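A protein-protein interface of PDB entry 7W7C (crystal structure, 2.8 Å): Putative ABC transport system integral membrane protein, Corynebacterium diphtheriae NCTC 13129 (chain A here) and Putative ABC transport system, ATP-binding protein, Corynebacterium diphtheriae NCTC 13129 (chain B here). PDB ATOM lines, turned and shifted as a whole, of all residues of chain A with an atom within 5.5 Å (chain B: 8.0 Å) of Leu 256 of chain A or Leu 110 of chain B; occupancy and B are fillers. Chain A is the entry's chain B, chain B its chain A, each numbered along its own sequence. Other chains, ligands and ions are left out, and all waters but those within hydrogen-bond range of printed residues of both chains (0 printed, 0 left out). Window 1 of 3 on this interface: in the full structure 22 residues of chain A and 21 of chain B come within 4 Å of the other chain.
The side-chain amide nitrogen of Asn 93 of chain B sits close to the guanidinium group of Arg 251 of chain A, 3.4 Å away.
The side-chain hydroxyl (OH) of Tyr 265 of chain A sits at hydrogen-bond distance from a ring nitrogen (ND1) of His 109 of chain B, 2.9 Å away.
The guanidinium group (NH1) of Arg 81 of chain B lies within hydrogen-bond range of the backbone carbonyl oxygen (O) of Ala 257 of chain A, at 2.8 Å.
NE of Arg 82 of chain B sits at hydrogen-bond distance from O of Gly 260 of chain A.
The backbone carbonyl oxygen (O) of Asn 93 of chain B sits at hydrogen-bond distance from the guanidinium group (NH1) of Arg 152 of chain B (2.7 Å).
The guanidinium group (NH1) of Arg 82 of chain B lies within salt-bridge range of the side-chain carboxylate (OE2) of Glu 83 of chain B (3.6 Å).
The backbone NH of Ala 261 of chain A is in hydrogen-bond range of the backbone carbonyl oxygen of Leu 256 of chain A (2.9 Å).
The backbone carbonyl oxygen of Arg 82 of chain B lies close to the guanidinium group of Arg 111 of chain B (3.5 Å).
The side-chain amide nitrogen (NE2) of Gln 103 of chain B lies within hydrogen-bond range of the backbone carbonyl oxygen (O) of Leu 95 of chain B (2.8 Å).
NH2 of Arg 81 of chain B sits at hydrogen-bond distance from OG1 of Thr 78 of chain B (3.3 Å).
Among the printed residues, merely in contact across the chains: Ala 258 of chain A with Arg 81 of chain B, Gly 260 of chain A with Thr 78 of chain B, Asp 252 of chain A with Leu 95 of chain B, Leu 259 of chain A with Phe 89 of chain B, Val 255 of chain A with Asn 93 of chain B, Leu 259 of chain A with Arg 82 of chain B, Ala 258 of chain A with Phe 87 of chain B, Tyr 265 of chain A with Leu 110 of chain B, Leu 259 of chain A with Arg 152 of chain B, Leu 259 of chain A with Arg 81 of chain B, Leu 256 of chain A with Leu 110 of chain B, Leu 259 of chain A with Phe 87 of chain B, Ala 261 of chain A with Thr 78 of chain B, Ala 258 of chain A with Phe 89 of chain B and Leu 259 of chain A with Thr 107 of chain B.
Of the printed residues of chain B, Arg 251 of chain A touches Asn 93.
Of chain B, only Leu 110 (3.9 Å) comes within 4 Å of Leu 256 of chain A.
Ala 257 of chain A touches just one residue of chain B: Arg 81.
Printed residues of chain B within 4 Å of Ala 258 of chain A: Arg 81 (3.3 Å), Phe 87 (3.6 Å) and Phe 89 (3.9 Å).
Glu 83 of chain B touches none of the printed residues of chain A.
Printed residues of chain A within 4 Å of Phe 87 of chain B: Ala 258 and Leu 259.
Printed residues of chain A within 4 Å of Leu 95 of chain B: Asp 252.
Gln 103 of chain B touches none of the printed residues of chain A.
Printed residues of chain A within 4 Å of Leu 110 of chain B: Leu 256 and Tyr 265.
The nearest printed residue of chain A that does not touch Leu 110 of chain B is Ala 261 of chain A (4.01 Å).
The nearest printed residue of chain A that does not touch Arg 82 of chain B is Ala 261 of chain A (5.0 Å).
Of the 14 printed residues of chain A, 10 touch a printed residue of chain B.
Printed residues of chain A that touch a printed residue of chain B: Arg 251, Asp 252, Val 255, Leu 256, Ala 257, Ala 258, Leu 259, Gly 260, Ala 261 and Tyr 265.
Hydrophobic or aromatic side chains of chain A that line the printed part of chain B: Val 255, Leu 256, Ala 258, Leu 259 and Tyr 265.
Of the 22 printed residues of chain B, 11 touch a printed residue of chain A.
Printed residues of chain B that touch a printed residue of chain A: Thr 78, Arg 81, Arg 82, Phe 87, Phe 89, Asn 93, Leu 95, Thr 107, His 109, Leu 110 and Arg 152.
Hydrophobic or aromatic side chains of chain B that line the printed part of chain A: Phe 87, Phe 89, Leu 95, His 109 and Leu 110.
Among the printed residues, no Asp or Glu carboxylate lies within 4 Å of a Lys or Arg side-chain nitrogen of the other chain.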
ATOM      1  N   LEU A   3     -10.851 -13.144 -32.637  1.00  0.00           N
ATOM      2  CA  LEU A   3      -9.972 -14.309 -32.625  1.00  0.00           C
ATOM      3  C   LEU A   3     -10.327 -15.292 -33.730  1.00  0.00           C
ATOM      4  O   LEU A   3      -9.445 -15.954 -34.279  1.00  0.00           O
ATOM      5  CB  LEU A   3     -10.028 -15.001 -31.263  1.00  0.00           C
ATOM      6  CG  LEU A   3      -9.121 -16.229 -31.129  1.00  0.00           C
ATOM      7  CD1 LEU A   3      -7.666 -15.862 -31.394  1.00  0.00           C
ATOM      8  CD2 LEU A   3      -9.267 -16.879 -29.766  1.00  0.00           C
ATOM      9  N   ARG A 251      -7.298 -24.480 -24.883  1.00  0.00           N
ATOM     10  CA  ARG A 251      -6.531 -23.637 -23.961  1.00  0.00           C
ATOM     11  C   ARG A 251      -6.656 -22.147 -24.275  1.00  0.00           C
ATOM     12  O   ARG A 251      -6.693 -21.328 -23.348  1.00  0.00           O
ATOM     13  CB  ARG A 251      -5.053 -24.036 -23.947  1.00  0.00           C
ATOM     14  CG  ARG A 251      -4.199 -23.085 -23.106  1.00  0.00           C
ATOM     15  CD  ARG A 251      -2.810 -23.622 -22.819  1.00  0.00           C
ATOM     16  NE  ARG A 251      -2.648 -23.945 -21.405  1.00  0.00           N
ATOM     17  CZ  ARG A 251      -2.201 -23.095 -20.483  1.00  0.00           C
ATOM     18  NH1 ARG A 251      -1.857 -21.861 -20.822  1.00  0.00           N
ATOM     19  NH2 ARG A 251      -2.094 -23.485 -19.220  1.00  0.00           N
ATOM     20  N   ASP A 252      -6.704 -21.765 -25.553  1.00  0.00           N
ATOM     21  CA  ASP A 252      -6.994 -20.370 -25.874  1.00  0.00           C
ATOM     22  C   ASP A 252      -8.352 -19.958 -25.316  1.00  0.00           C
ATOM     23  O   ASP A 252      -8.499 -18.863 -24.750  1.00  0.00           O
ATOM     24  CB  ASP A 252      -6.938 -20.150 -27.387  1.00  0.00           C
ATOM     25  CG  ASP A 252      -5.551 -20.367 -27.954  1.00  0.00           C
ATOM     26  OD1 ASP A 252      -4.617 -20.600 -27.158  1.00  0.00           O
ATOM     27  OD2 ASP A 252      -5.396 -20.313 -29.193  1.00  0.00           O
ATOM     28  N   ILE A 253      -9.349 -20.838 -25.447  1.00  0.00           N
ATOM     29  CA  ILE A 253     -10.670 -20.537 -24.895  1.00  0.00           C
ATOM     30  C   ILE A 253     -10.600 -20.407 -23.378  1.00  0.00           C
ATOM     31  O   ILE A 253     -11.271 -19.557 -22.776  1.00  0.00           O
ATOM     32  CB  ILE A 253     -11.689 -21.608 -25.331  1.00  0.00           C
ATOM     33  CG1 ILE A 253     -11.930 -21.511 -26.835  1.00  0.00           C
ATOM     34  CG2 ILE A 253     -12.999 -21.458 -24.558  1.00  0.00           C
ATOM     35  CD1 ILE A 253     -12.638 -22.714 -27.428  1.00  0.00           C
ATOM     36  N   ALA A 254      -9.778 -21.239 -22.739  1.00  0.00           N
ATOM     37  CA  ALA A 254      -9.628 -21.179 -21.288  1.00  0.00           C
ATOM     38  C   ALA A 254      -9.007 -19.858 -20.853  1.00  0.00           C
ATOM     39  O   ALA A 254      -9.439 -19.248 -19.867  1.00  0.00           O
ATOM     40  CB  ALA A 254      -8.785 -22.358 -20.804  1.00  0.00           C
ATOM     41  N   VAL A 255      -7.970 -19.420 -21.567  1.00  0.00           N
ATOM     42  CA  VAL A 255      -7.334 -18.136 -21.263  1.00  0.00           C
ATOM     43  C   VAL A 255      -8.347 -17.006 -21.386  1.00  0.00           C
ATOM     44  O   VAL A 255      -8.423 -16.111 -20.533  1.00  0.00           O
ATOM     45  CB  VAL A 255      -6.119 -17.897 -22.182  1.00  0.00           C
ATOM     46  CG1 VAL A 255      -5.596 -16.483 -21.998  1.00  0.00           C
ATOM     47  CG2 VAL A 255      -5.023 -18.917 -21.902  1.00  0.00           C
ATOM     48  N   LEU A 256      -9.137 -17.030 -22.463  1.00  0.00           N
ATOM     49  CA  LEU A 256     -10.141 -15.986 -22.660  1.00  0.00           C
ATOM     50  C   LEU A 256     -11.176 -15.982 -21.538  1.00  0.00           C
ATOM     51  O   LEU A 256     -11.542 -14.916 -21.019  1.00  0.00           O
ATOM     52  CB  LEU A 256     -10.814 -16.168 -24.018  1.00  0.00           C
ATOM     53  CG  LEU A 256      -9.973 -15.666 -25.190  1.00  0.00           C
ATOM     54  CD1 LEU A 256     -10.662 -15.950 -26.516  1.00  0.00           C
ATOM     55  CD2 LEU A 256      -9.671 -14.179 -25.041  1.00  0.00           C
ATOM     56  N   ALA A 257     -11.665 -17.165 -21.156  1.00  0.00           N
ATOM     57  CA  ALA A 257     -12.608 -17.259 -20.045  1.00  0.00           C
ATOM     58  C   ALA A 257     -12.008 -16.699 -18.762  1.00  0.00           C
ATOM     59  O   ALA A 257     -12.664 -15.941 -18.039  1.00  0.00           O
ATOM     60  CB  ALA A 257     -13.036 -18.713 -19.847  1.00  0.00           C
ATOM     61  N   ALA A 258     -10.757 -17.057 -18.468  1.00  0.00           N
ATOM     62  CA  ALA A 258     -10.086 -16.541 -17.279  1.00  0.00           C
ATOM     63  C   ALA A 258     -10.017 -15.021 -17.301  1.00  0.00           C
ATOM     64  O   ALA A 258     -10.306 -14.359 -16.299  1.00  0.00           O
ATOM     65  CB  ALA A 258      -8.681 -17.138 -17.174  1.00  0.00           C
ATOM     66  N   LEU A 259      -9.629 -14.449 -18.444  1.00  0.00           N
ATOM     67  CA  LEU A 259      -9.544 -12.997 -18.550  1.00  0.00           C
ATOM     68  C   LEU A 259     -10.907 -12.345 -18.385  1.00  0.00           C
ATOM     69  O   LEU A 259     -10.997 -11.206 -17.914  1.00  0.00           O
ATOM     70  CB  LEU A 259      -8.920 -12.593 -19.886  1.00  0.00           C
ATOM     71  CG  LEU A 259      -7.445 -12.950 -20.072  1.00  0.00           C
ATOM     72  CD1 LEU A 259      -6.858 -12.167 -21.234  1.00  0.00           C
ATOM     73  CD2 LEU A 259      -6.671 -12.677 -18.796  1.00  0.00           C
ATOM     74  N   GLY A 260     -11.971 -13.043 -18.764  1.00  0.00           N
ATOM     75  CA  GLY A 260     -13.296 -12.558 -18.428  1.00  0.00           C
ATOM     76  C   GLY A 260     -14.288 -12.567 -19.567  1.00  0.00           C
ATOM     77  O   GLY A 260     -15.357 -11.952 -19.476  1.00  0.00           O
ATOM     78  N   ALA A 261     -13.939 -13.260 -20.646  1.00  0.00           N
ATOM     79  CA  ALA A 261     -14.830 -13.367 -21.788  1.00  0.00           C
ATOM     80  C   ALA A 261     -16.084 -14.140 -21.412  1.00  0.00           C
ATOM     81  O   ALA A 261     -16.021 -15.165 -20.726  1.00  0.00           O
ATOM     82  CB  ALA A 261     -14.118 -14.053 -22.950  1.00  0.00           C
ATOM     83  N   TYR A 265     -20.041 -14.398 -25.656  1.00  0.00           N
ATOM     84  CA  TYR A 265     -18.946 -13.938 -26.504  1.00  0.00           C
ATOM     85  C   TYR A 265     -18.219 -15.106 -27.160  1.00  0.00           C
ATOM     86  O   TYR A 265     -18.017 -15.121 -28.382  1.00  0.00           O
ATOM     87  CB  TYR A 265     -17.980 -13.096 -25.671  1.00  0.00           C
ATOM     88  CG  TYR A 265     -16.764 -12.611 -26.419  1.00  0.00           C
ATOM     89  CD1 TYR A 265     -15.593 -13.357 -26.440  1.00  0.00           C
ATOM     90  CD2 TYR A 265     -16.783 -11.399 -27.092  1.00  0.00           C
ATOM     91  CE1 TYR A 265     -14.477 -12.917 -27.119  1.00  0.00           C
ATOM     92  CE2 TYR A 265     -15.671 -10.947 -27.769  1.00  0.00           C
ATOM     93  CZ  TYR A 265     -14.520 -11.710 -27.781  1.00  0.00           C
ATOM     94  OH  TYR A 265     -13.408 -11.267 -28.457  1.00  0.00           O
ATOM     95  N   LEU A 266     -17.799 -16.088 -26.356  1.00  0.00           N
ATOM     96  CA  LEU A 266     -17.073 -17.232 -26.907  1.00  0.00           C
ATOM     97  C   LEU A 266     -17.928 -18.004 -27.905  1.00  0.00           C
ATOM     98  O   LEU A 266     -17.432 -18.464 -28.944  1.00  0.00           O
ATOM     99  CB  LEU A 266     -16.612 -18.155 -25.780  1.00  0.00           C
ATOM    100  CG  LEU A 266     -15.708 -17.562 -24.700  1.00  0.00           C
ATOM    101  CD1 LEU A 266     -15.584 -18.532 -23.547  1.00  0.00           C
ATOM    102  CD2 LEU A 266     -14.339 -17.256 -25.282  1.00  0.00           C
ATOM    103  N   THR B  78     -17.179 -13.683 -13.351  1.00  0.00           N
ATOM    104  CA  THR B  78     -16.592 -13.450 -14.667  1.00  0.00           C
ATOM    105  C   THR B  78     -16.498 -11.962 -14.970  1.00  0.00           C
ATOM    106  O   THR B  78     -15.445 -11.466 -15.381  1.00  0.00           O
ATOM    107  CB  THR B  78     -17.406 -14.147 -15.756  1.00  0.00           C
ATOM    108  OG1 THR B  78     -17.392 -15.562 -15.545  1.00  0.00           O
ATOM    109  CG2 THR B  78     -16.816 -13.835 -17.121  1.00  0.00           C
ATOM    110  N   ARG B  81     -13.780 -10.216 -13.006  1.00  0.00           N
ATOM    111  CA  ARG B  81     -12.501 -10.347 -13.700  1.00  0.00           C
ATOM    112  C   ARG B  81     -12.429  -9.415 -14.906  1.00  0.00           C
ATOM    113  O   ARG B  81     -11.474  -8.643 -15.060  1.00  0.00           O
ATOM    114  CB  ARG B  81     -12.289 -11.798 -14.137  1.00  0.00           C
ATOM    115  CG  ARG B  81     -12.330 -12.795 -12.998  1.00  0.00           C
ATOM    116  CD  ARG B  81     -12.006 -14.207 -13.469  1.00  0.00           C
ATOM    117  NE  ARG B  81     -13.099 -15.130 -13.187  1.00  0.00           N
ATOM    118  CZ  ARG B  81     -13.825 -15.747 -14.117  1.00  0.00           C
ATOM    119  NH1 ARG B  81     -13.557 -15.560 -15.402  1.00  0.00           N
ATOM    120  NH2 ARG B  81     -14.808 -16.566 -13.759  1.00  0.00           N
ATOM    121  N   ARG B  82     -13.452  -9.461 -15.763  1.00  0.00           N
ATOM    122  CA  ARG B  82     -13.450  -8.734 -17.029  1.00  0.00           C
ATOM    123  C   ARG B  82     -13.394  -7.224 -16.849  1.00  0.00           C
ATOM    124  O   ARG B  82     -12.911  -6.521 -17.744  1.00  0.00           O
ATOM    125  CB  ARG B  82     -14.695  -9.103 -17.840  1.00  0.00           C
ATOM    126  CG  ARG B  82     -14.733  -8.506 -19.242  1.00  0.00           C
ATOM    127  CD  ARG B  82     -16.147  -8.230 -19.715  1.00  0.00           C
ATOM    128  NE  ARG B  82     -17.038  -9.368 -19.512  1.00  0.00           N
ATOM    129  CZ  ARG B  82     -18.159  -9.317 -18.798  1.00  0.00           C
ATOM    130  NH1 ARG B  82     -18.536  -8.181 -18.230  1.00  0.00           N
ATOM    131  NH2 ARG B  82     -18.915 -10.398 -18.663  1.00  0.00           N
ATOM    132  N   GLU B  83     -13.875  -6.708 -15.721  1.00  0.00           N
ATOM    133  CA  GLU B  83     -13.968  -5.274 -15.522  1.00  0.00           C
ATOM    134  C   GLU B  83     -12.990  -4.723 -14.493  1.00  0.00           C
ATOM    135  O   GLU B  83     -12.794  -3.503 -14.457  1.00  0.00           O
ATOM    136  CB  GLU B  83     -15.402  -4.901 -15.119  1.00  0.00           C
ATOM    137  CG  GLU B  83     -16.439  -5.344 -16.137  1.00  0.00           C
ATOM    138  CD  GLU B  83     -17.826  -4.769 -15.873  1.00  0.00           C
ATOM    139  OE1 GLU B  83     -18.021  -4.113 -14.825  1.00  0.00           O
ATOM    140  OE2 GLU B  83     -18.723  -4.970 -16.725  1.00  0.00           O
ATOM    141  N   PHE B  87      -4.388 -10.354 -15.016  1.00  0.00           N
ATOM    142  CA  PHE B  87      -3.861 -11.687 -14.723  1.00  0.00           C
ATOM    143  C   PHE B  87      -2.497 -11.878 -15.381  1.00  0.00           C
ATOM    144  O   PHE B  87      -2.419 -12.183 -16.575  1.00  0.00           O
ATOM    145  CB  PHE B  87      -4.830 -12.766 -15.204  1.00  0.00           C
ATOM    146  CG  PHE B  87      -6.167 -12.746 -14.523  1.00  0.00           C
ATOM    147  CD1 PHE B  87      -7.190 -11.955 -15.009  1.00  0.00           C
ATOM    148  CD2 PHE B  87      -6.402 -13.531 -13.405  1.00  0.00           C
ATOM    149  CE1 PHE B  87      -8.425 -11.935 -14.392  1.00  0.00           C
ATOM    150  CE2 PHE B  87      -7.639 -13.516 -12.780  1.00  0.00           C
ATOM    151  CZ  PHE B  87      -8.650 -12.719 -13.276  1.00  0.00           C
ATOM    152  N   PHE B  89      -0.332 -14.403 -15.672  1.00  0.00           N
ATOM    153  CA  PHE B  89      -0.288 -15.844 -15.485  1.00  0.00           C
ATOM    154  C   PHE B  89       1.152 -16.335 -15.406  1.00  0.00           C
ATOM    155  O   PHE B  89       2.092 -15.675 -15.872  1.00  0.00           O
ATOM    156  CB  PHE B  89      -0.983 -16.563 -16.636  1.00  0.00           C
ATOM    157  CG  PHE B  89      -2.425 -16.191 -16.821  1.00  0.00           C
ATOM    158  CD1 PHE B  89      -3.412 -16.793 -16.056  1.00  0.00           C
ATOM    159  CD2 PHE B  89      -2.791 -15.272 -17.791  1.00  0.00           C
ATOM    160  CE1 PHE B  89      -4.738 -16.470 -16.234  1.00  0.00           C
ATOM    161  CE2 PHE B  89      -4.116 -14.945 -17.983  1.00  0.00           C
ATOM    162  CZ  PHE B  89      -5.094 -15.544 -17.201  1.00  0.00           C
ATOM    163  N   ASN B  93       0.671 -17.429 -21.673  1.00  0.00           N
ATOM    164  CA  ASN B  93      -0.712 -17.607 -22.138  1.00  0.00           C
ATOM    165  C   ASN B  93      -1.078 -16.584 -23.212  1.00  0.00           C
ATOM    166  O   ASN B  93      -2.087 -15.883 -23.126  1.00  0.00           O
ATOM    167  CB  ASN B  93      -1.697 -17.552 -20.966  1.00  0.00           C
ATOM    168  CG  ASN B  93      -1.746 -18.849 -20.183  1.00  0.00           C
ATOM    169  OD1 ASN B  93      -0.974 -19.769 -20.441  1.00  0.00           O
ATOM    170  ND2 ASN B  93      -2.648 -18.921 -19.207  1.00  0.00           N
ATOM    171  N   LEU B  95      -2.001 -15.914 -27.267  1.00  0.00           N
ATOM    172  CA  LEU B  95      -2.762 -16.617 -28.288  1.00  0.00           C
ATOM    173  C   LEU B  95      -1.982 -16.578 -29.597  1.00  0.00           C
ATOM    174  O   LEU B  95      -1.651 -15.497 -30.097  1.00  0.00           O
ATOM    175  CB  LEU B  95      -4.147 -15.992 -28.429  1.00  0.00           C
ATOM    176  CG  LEU B  95      -4.868 -15.906 -27.078  1.00  0.00           C
ATOM    177  CD1 LEU B  95      -6.297 -15.390 -27.238  1.00  0.00           C
ATOM    178  CD2 LEU B  95      -4.834 -17.244 -26.329  1.00  0.00           C
ATOM    179  N   LEU B  98      -2.498 -14.350 -32.763  1.00  0.00           N
ATOM    180  CA  LEU B  98      -2.494 -12.911 -32.571  1.00  0.00           C
ATOM    181  C   LEU B  98      -1.072 -12.372 -32.506  1.00  0.00           C
ATOM    182  O   LEU B  98      -0.143 -13.049 -32.052  1.00  0.00           O
ATOM    183  CB  LEU B  98      -3.252 -12.544 -31.295  1.00  0.00           C
ATOM    184  CG  LEU B  98      -4.702 -13.025 -31.235  1.00  0.00           C
ATOM    185  CD1 LEU B  98      -5.337 -12.685 -29.895  1.00  0.00           C
ATOM    186  CD2 LEU B  98      -5.490 -12.407 -32.362  1.00  0.00           C
ATOM    187  N   GLN B 103      -2.570  -9.197 -28.653  1.00  0.00           N
ATOM    188  CA  GLN B 103      -2.746  -9.747 -27.310  1.00  0.00           C
ATOM    189  C   GLN B 103      -3.355  -8.710 -26.376  1.00  0.00           C
ATOM    190  O   GLN B 103      -4.188  -9.043 -25.524  1.00  0.00           O
ATOM    191  CB  GLN B 103      -1.408 -10.236 -26.749  1.00  0.00           C
ATOM    192  CG  GLN B 103      -0.567 -11.087 -27.697  1.00  0.00           C
ATOM    193  CD  GLN B 103      -1.091 -12.501 -27.856  1.00  0.00           C
ATOM    194  OE1 GLN B 103      -1.890 -12.972 -27.045  1.00  0.00           O
ATOM    195  NE2 GLN B 103      -0.642 -13.189 -28.901  1.00  0.00           N
ATOM    196  N   LEU B 104      -2.954  -7.446 -26.524  1.00  0.00           N
ATOM    197  CA  LEU B 104      -3.539  -6.381 -25.719  1.00  0.00           C
ATOM    198  C   LEU B 104      -4.910  -5.983 -26.251  1.00  0.00           C
ATOM    199  O   LEU B 104      -5.865  -5.841 -25.480  1.00  0.00           O
ATOM    200  CB  LEU B 104      -2.600  -5.170 -25.681  1.00  0.00           C
ATOM    201  CG  LEU B 104      -1.500  -5.161 -24.614  1.00  0.00           C
ATOM    202  CD1 LEU B 104      -0.595  -6.376 -24.722  1.00  0.00           C
ATOM    203  CD2 LEU B 104      -0.675  -3.890 -24.690  1.00  0.00           C
ATOM    204  N   LEU B 105      -5.029  -5.836 -27.576  1.00  0.00           N
ATOM    205  CA  LEU B 105      -6.257  -5.292 -28.156  1.00  0.00           C
ATOM    206  C   LEU B 105      -7.463  -6.203 -27.910  1.00  0.00           C
ATOM    207  O   LEU B 105      -8.593  -5.720 -27.740  1.00  0.00           O
ATOM    208  CB  LEU B 105      -6.074  -5.056 -29.654  1.00  0.00           C
ATOM    209  CG  LEU B 105      -5.123  -3.928 -30.062  1.00  0.00           C
ATOM    210  CD1 LEU B 105      -4.822  -4.004 -31.546  1.00  0.00           C
ATOM    211  CD2 LEU B 105      -5.704  -2.572 -29.699  1.00  0.00           C
ATOM    212  N   ILE B 106      -7.253  -7.523 -27.892  1.00  0.00           N
ATOM    213  CA  ILE B 106      -8.415  -8.400 -27.767  1.00  0.00           C
ATOM    214  C   ILE B 106      -9.077  -8.239 -26.400  1.00  0.00           C
ATOM    215  O   ILE B 106     -10.284  -8.467 -26.261  1.00  0.00           O
ATOM    216  CB  ILE B 106      -8.052  -9.873 -28.054  1.00  0.00           C
ATOM    217  CG1 ILE B 106      -9.335 -10.709 -28.177  1.00  0.00           C
ATOM    218  CG2 ILE B 106      -7.134 -10.432 -26.975  1.00  0.00           C
ATOM    219  CD1 ILE B 106      -9.107 -12.147 -28.604  1.00  0.00           C
ATOM    220  N   THR B 107      -8.327  -7.813 -25.376  1.00  0.00           N
ATOM    221  CA  THR B 107      -8.967  -7.579 -24.086  1.00  0.00           C
ATOM    222  C   THR B 107      -9.847  -6.334 -24.121  1.00  0.00           C
ATOM    223  O   THR B 107     -10.809  -6.239 -23.348  1.00  0.00           O
ATOM    224  CB  THR B 107      -7.928  -7.459 -22.977  1.00  0.00           C
ATOM    225  OG1 THR B 107      -7.161  -6.262 -23.159  1.00  0.00           O
ATOM    226  CG2 THR B 107      -7.007  -8.663 -22.997  1.00  0.00           C
ATOM    227  N   ASP B 108      -9.533  -5.374 -24.998  1.00  0.00           N
ATOM    228  CA  ASP B 108     -10.495  -4.320 -25.302  1.00  0.00           C
ATOM    229  C   ASP B 108     -11.717  -4.895 -25.994  1.00  0.00           C
ATOM    230  O   ASP B 108     -12.853  -4.527 -25.675  1.00  0.00           O
ATOM    231  CB  ASP B 108      -9.857  -3.248 -26.180  1.00  0.00           C
ATOM    232  CG  ASP B 108      -9.246  -2.119 -25.381  1.00  0.00           C
ATOM    233  OD1 ASP B 108      -9.130  -2.243 -24.146  1.00  0.00           O
ATOM    234  OD2 ASP B 108      -8.882  -1.095 -25.992  1.00  0.00           O
ATOM    235  N   HIS B 109     -11.498  -5.816 -26.939  1.00  0.00           N
ATOM    236  CA  HIS B 109     -12.612  -6.352 -27.719  1.00  0.00           C
ATOM    237  C   HIS B 109     -13.638  -7.046 -26.827  1.00  0.00           C
ATOM    238  O   HIS B 109     -14.826  -6.704 -26.846  1.00  0.00           O
ATOM    239  CB  HIS B 109     -12.096  -7.314 -28.788  1.00  0.00           C
ATOM    240  CG  HIS B 109     -13.140  -7.711 -29.784  1.00  0.00           C
ATOM    241  ND1 HIS B 109     -14.082  -8.684 -29.531  1.00  0.00           N
ATOM    242  CD2 HIS B 109     -13.397  -7.255 -31.033  1.00  0.00           C
ATOM    243  CE1 HIS B 109     -14.873  -8.812 -30.581  1.00  0.00           C
ATOM    244  NE2 HIS B 109     -14.479  -7.956 -31.506  1.00  0.00           N
ATOM    245  N   LEU B 110     -13.199  -8.028 -26.037  1.00  0.00           N
ATOM    246  CA  LEU B 110     -14.126  -8.770 -25.186  1.00  0.00           C
ATOM    247  C   LEU B 110     -14.709  -7.909 -24.073  1.00  0.00           C
ATOM    248  O   LEU B 110     -15.728  -8.290 -23.485  1.00  0.00           O
ATOM    249  CB  LEU B 110     -13.433 -10.003 -24.596  1.00  0.00           C
ATOM    250  CG  LEU B 110     -12.312  -9.822 -23.568  1.00  0.00           C
ATOM    251  CD1 LEU B 110     -12.828  -9.711 -22.135  1.00  0.00           C
ATOM    252  CD2 LEU B 110     -11.300 -10.959 -23.684  1.00  0.00           C
ATOM    253  N   ARG B 111     -14.076  -6.778 -23.755  1.00  0.00           N
ATOM    254  CA  ARG B 111     -14.641  -5.797 -22.835  1.00  0.00           C
ATOM    255  C   ARG B 111     -15.732  -4.951 -23.472  1.00  0.00           C
ATOM    256  O   ARG B 111     -16.311  -4.100 -22.788  1.00  0.00           O
ATOM    257  CB  ARG B 111     -13.547  -4.883 -22.285  1.00  0.00           C
ATOM    258  CG  ARG B 111     -13.037  -5.280 -20.916  1.00  0.00           C
ATOM    259  CD  ARG B 111     -11.897  -4.379 -20.461  1.00  0.00           C
ATOM    260  NE  ARG B 111     -10.719  -5.156 -20.084  1.00  0.00           N
ATOM    261  CZ  ARG B 111      -9.528  -5.063 -20.667  1.00  0.00           C
ATOM    262  NH1 ARG B 111      -9.331  -4.194 -21.655  1.00  0.00           N
ATOM    263  NH2 ARG B 111      -8.525  -5.822 -20.242  1.00  0.00           N
ATOM    264  N   GLY B 112     -16.012  -5.149 -24.759  1.00  0.00           N
ATOM    265  CA  GLY B 112     -17.125  -4.503 -25.419  1.00  0.00           C
ATOM    266  C   GLY B 112     -16.798  -3.266 -26.228  1.00  0.00           C
ATOM    267  O   GLY B 112     -17.686  -2.755 -26.920  1.00  0.00           O
ATOM    268  N   ILE B 113     -15.561  -2.778 -26.187  1.00  0.00           N
ATOM    269  CA  ILE B 113     -15.237  -1.468 -26.735  1.00  0.00           C
ATOM    270  C   ILE B 113     -14.303  -1.603 -27.934  1.00  0.00           C
ATOM    271  O   ILE B 113     -13.619  -2.612 -28.124  1.00  0.00           O
ATOM    272  CB  ILE B 113     -14.629  -0.545 -25.660  1.00  0.00           C
ATOM    273  CG1 ILE B 113     -13.221  -1.012 -25.278  1.00  0.00           C
ATOM    274  CG2 ILE B 113     -15.532  -0.508 -24.436  1.00  0.00           C
ATOM    275  CD1 ILE B 113     -12.118  -0.032 -25.643  1.00  0.00           C
ATOM    276  N   PRO B 115     -11.164  -1.452 -29.997  1.00  0.00           N
ATOM    277  CA  PRO B 115      -9.778  -1.551 -29.519  1.00  0.00           C
ATOM    278  C   PRO B 115      -8.963  -0.293 -29.783  1.00  0.00           C
ATOM    279  O   PRO B 115      -9.037   0.310 -30.856  1.00  0.00           O
ATOM    280  CB  PRO B 115      -9.229  -2.747 -30.299  1.00  0.00           C
ATOM    281  CG  PRO B 115     -10.432  -3.596 -30.529  1.00  0.00           C
ATOM    282  CD  PRO B 115     -11.564  -2.637 -30.774  1.00  0.00           C
ATOM    283  N   ARG B 152      -0.747  -6.806 -21.316  1.00  0.00           N
ATOM    284  CA  ARG B 152      -2.133  -7.227 -21.478  1.00  0.00           C
ATOM    285  C   ARG B 152      -2.913  -7.035 -20.187  1.00  0.00           C
ATOM    286  O   ARG B 152      -4.044  -6.536 -20.205  1.00  0.00           O
ATOM    287  CB  ARG B 152      -2.194  -8.690 -21.918  1.00  0.00           C
ATOM    288  CG  ARG B 152      -3.595  -9.281 -21.875  1.00  0.00           C
ATOM    289  CD  ARG B 152      -3.617 -10.708 -22.399  1.00  0.00           C
ATOM    290  NE  ARG B 152      -2.812 -11.606 -21.578  1.00  0.00           N
ATOM    291  CZ  ARG B 152      -2.549 -12.870 -21.893  1.00  0.00           C
ATOM    292  NH1 ARG B 152      -3.025 -13.380 -23.022  1.00  0.00           N
ATOM    293  NH2 ARG B 152      -1.803 -13.617 -21.088  1.00  0.00           N
